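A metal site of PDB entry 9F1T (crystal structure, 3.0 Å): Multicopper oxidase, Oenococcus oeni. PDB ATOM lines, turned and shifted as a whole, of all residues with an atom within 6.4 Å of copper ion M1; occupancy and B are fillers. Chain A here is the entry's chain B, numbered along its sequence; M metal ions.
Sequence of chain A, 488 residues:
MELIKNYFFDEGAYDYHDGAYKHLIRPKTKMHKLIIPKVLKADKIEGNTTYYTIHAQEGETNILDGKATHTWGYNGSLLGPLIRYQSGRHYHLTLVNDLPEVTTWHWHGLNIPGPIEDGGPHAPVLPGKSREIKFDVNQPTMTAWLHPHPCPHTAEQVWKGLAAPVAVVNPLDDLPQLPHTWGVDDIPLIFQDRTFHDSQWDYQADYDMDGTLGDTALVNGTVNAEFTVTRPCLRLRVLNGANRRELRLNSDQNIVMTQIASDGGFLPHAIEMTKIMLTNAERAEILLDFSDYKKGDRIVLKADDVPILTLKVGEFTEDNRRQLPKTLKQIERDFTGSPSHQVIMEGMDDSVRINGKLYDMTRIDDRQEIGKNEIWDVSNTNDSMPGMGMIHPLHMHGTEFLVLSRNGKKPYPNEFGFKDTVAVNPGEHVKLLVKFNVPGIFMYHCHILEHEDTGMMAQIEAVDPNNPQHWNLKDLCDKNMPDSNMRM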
ATOM      1  N   HIS A 106     -18.757  19.765  -0.235  1.00  0.00           N
ATOM      2  CA  HIS A 106     -18.044  19.525   1.001  1.00  0.00           C
ATOM      3  C   HIS A 106     -18.988  18.874   2.004  1.00  0.00           C
ATOM      4  O   HIS A 106     -20.045  19.421   2.294  1.00  0.00           O
ATOM      5  CB  HIS A 106     -17.440  20.805   1.589  1.00  0.00           C
ATOM      6  CG  HIS A 106     -16.789  20.533   2.908  1.00  0.00           C
ATOM      7  ND1 HIS A 106     -16.176  19.334   3.170  1.00  0.00           N
ATOM      8  CD2 HIS A 106     -16.665  21.267   4.018  1.00  0.00           C
ATOM      9  CE1 HIS A 106     -15.702  19.346   4.401  1.00  0.00           C
ATOM     10  NE2 HIS A 106     -15.985  20.515   4.934  1.00  0.00           N
ATOM     11  N   HIS A 108     -19.118  18.498   5.355  1.00  0.00           N
ATOM     12  CA  HIS A 108     -18.645  19.019   6.634  1.00  0.00           C
ATOM     13  C   HIS A 108     -19.082  18.083   7.759  1.00  0.00           C
ATOM     14  O   HIS A 108     -20.256  18.078   8.131  1.00  0.00           O
ATOM     15  CB  HIS A 108     -19.190  20.443   6.856  1.00  0.00           C
ATOM     16  CG  HIS A 108     -18.786  21.035   8.148  1.00  0.00           C
ATOM     17  ND1 HIS A 108     -18.397  22.350   8.225  1.00  0.00           N
ATOM     18  CD2 HIS A 108     -18.691  20.547   9.400  1.00  0.00           C
ATOM     19  CE1 HIS A 108     -18.069  22.634   9.491  1.00  0.00           C
ATOM     20  NE2 HIS A 108     -18.247  21.550  10.209  1.00  0.00           N
ATOM     21  N   GLY A 109     -18.129  17.312   8.283  1.00  0.00           N
ATOM     22  CA  GLY A 109     -18.396  16.405   9.389  1.00  0.00           C
ATOM     23  C   GLY A 109     -17.967  14.980   9.063  1.00  0.00           C
ATOM     24  O   GLY A 109     -17.527  14.260   9.966  1.00  0.00           O
ATOM     25  N   TRP A 145     -23.306  18.015   7.946  1.00  0.00           N
ATOM     26  CA  TRP A 145     -24.031  18.702   6.890  1.00  0.00           C
ATOM     27  C   TRP A 145     -23.203  18.807   5.610  1.00  0.00           C
ATOM     28  O   TRP A 145     -21.985  18.652   5.636  1.00  0.00           O
ATOM     29  CB  TRP A 145     -24.516  20.091   7.345  1.00  0.00           C
ATOM     30  CG  TRP A 145     -23.438  21.053   7.780  1.00  0.00           C
ATOM     31  CD1 TRP A 145     -22.398  20.808   8.628  1.00  0.00           C
ATOM     32  CD2 TRP A 145     -23.324  22.433   7.378  1.00  0.00           C
ATOM     33  NE1 TRP A 145     -21.641  21.946   8.780  1.00  0.00           N
ATOM     34  CE2 TRP A 145     -22.179  22.958   8.032  1.00  0.00           C
ATOM     35  CE3 TRP A 145     -24.069  23.276   6.550  1.00  0.00           C
ATOM     36  CZ2 TRP A 145     -21.771  24.278   7.866  1.00  0.00           C
ATOM     37  CZ3 TRP A 145     -23.663  24.588   6.390  1.00  0.00           C
ATOM     38  CH2 TRP A 145     -22.535  25.080   7.046  1.00  0.00           C
ATOM     39  N   HIS A 147     -22.333  21.264   2.223  1.00  0.00           N
ATOM     40  CA  HIS A 147     -22.361  22.596   1.651  1.00  0.00           C
ATOM     41  C   HIS A 147     -21.297  22.696   0.574  1.00  0.00           C
ATOM     42  O   HIS A 147     -20.361  21.905   0.526  1.00  0.00           O
ATOM     43  CB  HIS A 147     -22.241  23.665   2.745  1.00  0.00           C
ATOM     44  CG  HIS A 147     -20.891  23.789   3.390  1.00  0.00           C
ATOM     45  ND1 HIS A 147     -19.849  24.536   2.902  1.00  0.00           N
ATOM     46  CD2 HIS A 147     -20.477  23.284   4.556  1.00  0.00           C
ATOM     47  CE1 HIS A 147     -18.828  24.461   3.739  1.00  0.00           C
ATOM     48  NE2 HIS A 147     -19.197  23.712   4.759  1.00  0.00           N
ATOM     49  N   HIS A 149     -18.036  24.334  -1.356  1.00  0.00           N
ATOM     50  CA  HIS A 149     -16.782  24.898  -0.890  1.00  0.00           C
ATOM     51  C   HIS A 149     -15.848  25.318  -2.029  1.00  0.00           C
ATOM     52  O   HIS A 149     -14.655  25.050  -1.955  1.00  0.00           O
ATOM     53  CB  HIS A 149     -16.027  23.851  -0.077  1.00  0.00           C
ATOM     54  CG  HIS A 149     -15.231  24.389   1.062  1.00  0.00           C
ATOM     55  ND1 HIS A 149     -14.432  25.507   0.949  1.00  0.00           N
ATOM     56  CD2 HIS A 149     -15.073  23.948   2.328  1.00  0.00           C
ATOM     57  CE1 HIS A 149     -13.838  25.737   2.114  1.00  0.00           C
ATOM     58  NE2 HIS A 149     -14.212  24.799   2.956  1.00  0.00           N
ATOM     59  N   ALA A 281     -21.187  26.783  11.777  1.00  0.00           N
ATOM     60  CA  ALA A 281     -20.812  25.405  11.472  1.00  0.00           C
ATOM     61  C   ALA A 281     -20.920  24.495  12.694  1.00  0.00           C
ATOM     62  O   ALA A 281     -20.729  23.286  12.592  1.00  0.00           O
ATOM     63  CB  ALA A 281     -19.440  25.342  10.833  1.00  0.00           C
ATOM     64  N   HIS A 395     -12.561  25.336  11.997  1.00  0.00           N
ATOM     65  CA  HIS A 395     -13.040  24.065  11.495  1.00  0.00           C
ATOM     66  C   HIS A 395     -11.870  23.292  10.879  1.00  0.00           C
ATOM     67  O   HIS A 395     -11.024  23.904  10.225  1.00  0.00           O
ATOM     68  CB  HIS A 395     -14.132  24.297  10.440  1.00  0.00           C
ATOM     69  CG  HIS A 395     -14.607  23.033   9.787  1.00  0.00           C
ATOM     70  ND1 HIS A 395     -14.860  21.884  10.497  1.00  0.00           N
ATOM     71  CD2 HIS A 395     -14.862  22.745   8.509  1.00  0.00           C
ATOM     72  CE1 HIS A 395     -15.247  20.931   9.656  1.00  0.00           C
ATOM     73  NE2 HIS A 395     -15.256  21.437   8.455  1.00  0.00           N
ATOM     74  N   HIS A 397     -11.227  19.866   8.397  1.00  0.00           N
ATOM     75  CA  HIS A 397     -11.772  18.840   7.526  1.00  0.00           C
ATOM     76  C   HIS A 397     -11.207  17.475   7.909  1.00  0.00           C
ATOM     77  O   HIS A 397     -10.078  17.368   8.377  1.00  0.00           O
ATOM     78  CB  HIS A 397     -11.443  19.095   6.046  1.00  0.00           C
ATOM     79  CG  HIS A 397     -12.089  20.285   5.426  1.00  0.00           C
ATOM     80  ND1 HIS A 397     -12.302  20.332   4.069  1.00  0.00           N
ATOM     81  CD2 HIS A 397     -12.522  21.461   5.900  1.00  0.00           C
ATOM     82  CE1 HIS A 397     -12.859  21.491   3.746  1.00  0.00           C
ATOM     83  NE2 HIS A 397     -12.999  22.199   4.846  1.00  0.00           N
ATOM     84  N   THR A 421     -15.640  21.849  14.845  1.00  0.00           N
ATOM     85  CA  THR A 421     -15.607  23.306  14.826  1.00  0.00           C
ATOM     86  C   THR A 421     -15.523  23.809  16.269  1.00  0.00           C
ATOM     87  O   THR A 421     -16.148  23.241  17.162  1.00  0.00           O
ATOM     88  CB  THR A 421     -16.844  23.859  14.103  1.00  0.00           C
ATOM     89  OG1 THR A 421     -16.890  23.237  12.818  1.00  0.00           O
ATOM     90  CG2 THR A 421     -16.788  25.361  13.891  1.00  0.00           C
ATOM     91  N   HIS A 445      -9.702  26.089   8.649  1.00  0.00           N
ATOM     92  CA  HIS A 445     -10.027  27.479   8.346  1.00  0.00           C
ATOM     93  C   HIS A 445     -11.075  28.048   9.288  1.00  0.00           C
ATOM     94  O   HIS A 445     -11.749  27.318  10.018  1.00  0.00           O
ATOM     95  CB  HIS A 445     -10.556  27.599   6.904  1.00  0.00           C
ATOM     96  CG  HIS A 445     -11.836  26.874   6.650  1.00  0.00           C
ATOM     97  ND1 HIS A 445     -13.004  27.549   6.400  1.00  0.00           N
ATOM     98  CD2 HIS A 445     -12.158  25.564   6.602  1.00  0.00           C
ATOM     99  CE1 HIS A 445     -13.990  26.691   6.201  1.00  0.00           C
ATOM    100  NE2 HIS A 445     -13.498  25.474   6.337  1.00  0.00           N
ATOM    101  N   HIS A 447     -14.624  29.521   9.745  1.00  0.00           N
ATOM    102  CA  HIS A 447     -15.859  29.148   9.082  1.00  0.00           C
ATOM    103  C   HIS A 447     -16.836  30.316   9.007  1.00  0.00           C
ATOM    104  O   HIS A 447     -18.011  30.128   8.713  1.00  0.00           O
ATOM    105  CB  HIS A 447     -16.497  27.934   9.773  1.00  0.00           C
ATOM    106  CG  HIS A 447     -17.244  27.076   8.811  1.00  0.00           C
ATOM    107  ND1 HIS A 447     -18.472  27.432   8.303  1.00  0.00           N
ATOM    108  CD2 HIS A 447     -16.929  25.913   8.232  1.00  0.00           C
ATOM    109  CE1 HIS A 447     -18.878  26.489   7.467  1.00  0.00           C
ATOM    110  NE2 HIS A 447     -17.952  25.556   7.405  1.00  0.00           N
ATOM    111  N   LEU A 449     -17.632  32.712   6.458  1.00  0.00           N
ATOM    112  CA  LEU A 449     -17.413  32.300   5.085  1.00  0.00           C
ATOM    113  C   LEU A 449     -16.696  33.397   4.296  1.00  0.00           C
ATOM    114  O   LEU A 449     -16.022  33.093   3.320  1.00  0.00           O
ATOM    115  CB  LEU A 449     -18.755  31.916   4.451  1.00  0.00           C
ATOM    116  CG  LEU A 449     -19.514  30.763   5.110  1.00  0.00           C
ATOM    117  CD1 LEU A 449     -20.707  30.346   4.281  1.00  0.00           C
ATOM    118  CD2 LEU A 449     -18.599  29.569   5.371  1.00  0.00           C
HETATM  119 CU    CU M   1     -18.158  23.448   6.667  1.00  0.00          CU
HETATM  120 CU    CU M   2     -15.420  20.787   6.761  1.00  0.00          CU
HETATM  121 CU    CU M   3     -14.145  23.663   4.828  1.00  0.00          CU
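His 106 touches copper ion M1 (CD2 to CU, 3.7 Å). Trp 145 touches copper ion M1 (CZ2 to CU, 3.9 Å). His 395 touches copper ion M1. Within 4 Å of copper ion M1: His 106, His 108, Trp 145, His 147, His 395 and His 447. The nearest printed residue that does not touch copper ion M1 is Ala 281 (4.8 Å).
NE2 of His 108 lies close to ND1 of His 395. O of Trp 145 is in hydrogen-bond range of N of His 108 (2.9 Å). NE2 of His 108 sits at hydrogen-bond distance from OG1 of Thr 421 (3.4 Å). N of His 106 lies within hydrogen-bond range of O of His 147 (2.8 Å). The backbone carbonyl oxygen (O) of His 445 sits at hydrogen-bond distance from the backbone NH (N) of His 395 (2.9 Å). OG1 of Thr 421 is in hydrogen-bond range of ND1 of His 395.
A ring nitrogen (ND1) of His 108 binds copper ion M1 (1.9 Å). NE2 of His 147 binds copper ion M1 (2.2 Å). Copper ion M1 is bound by NE2 of His 447, 2.2 Å away.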
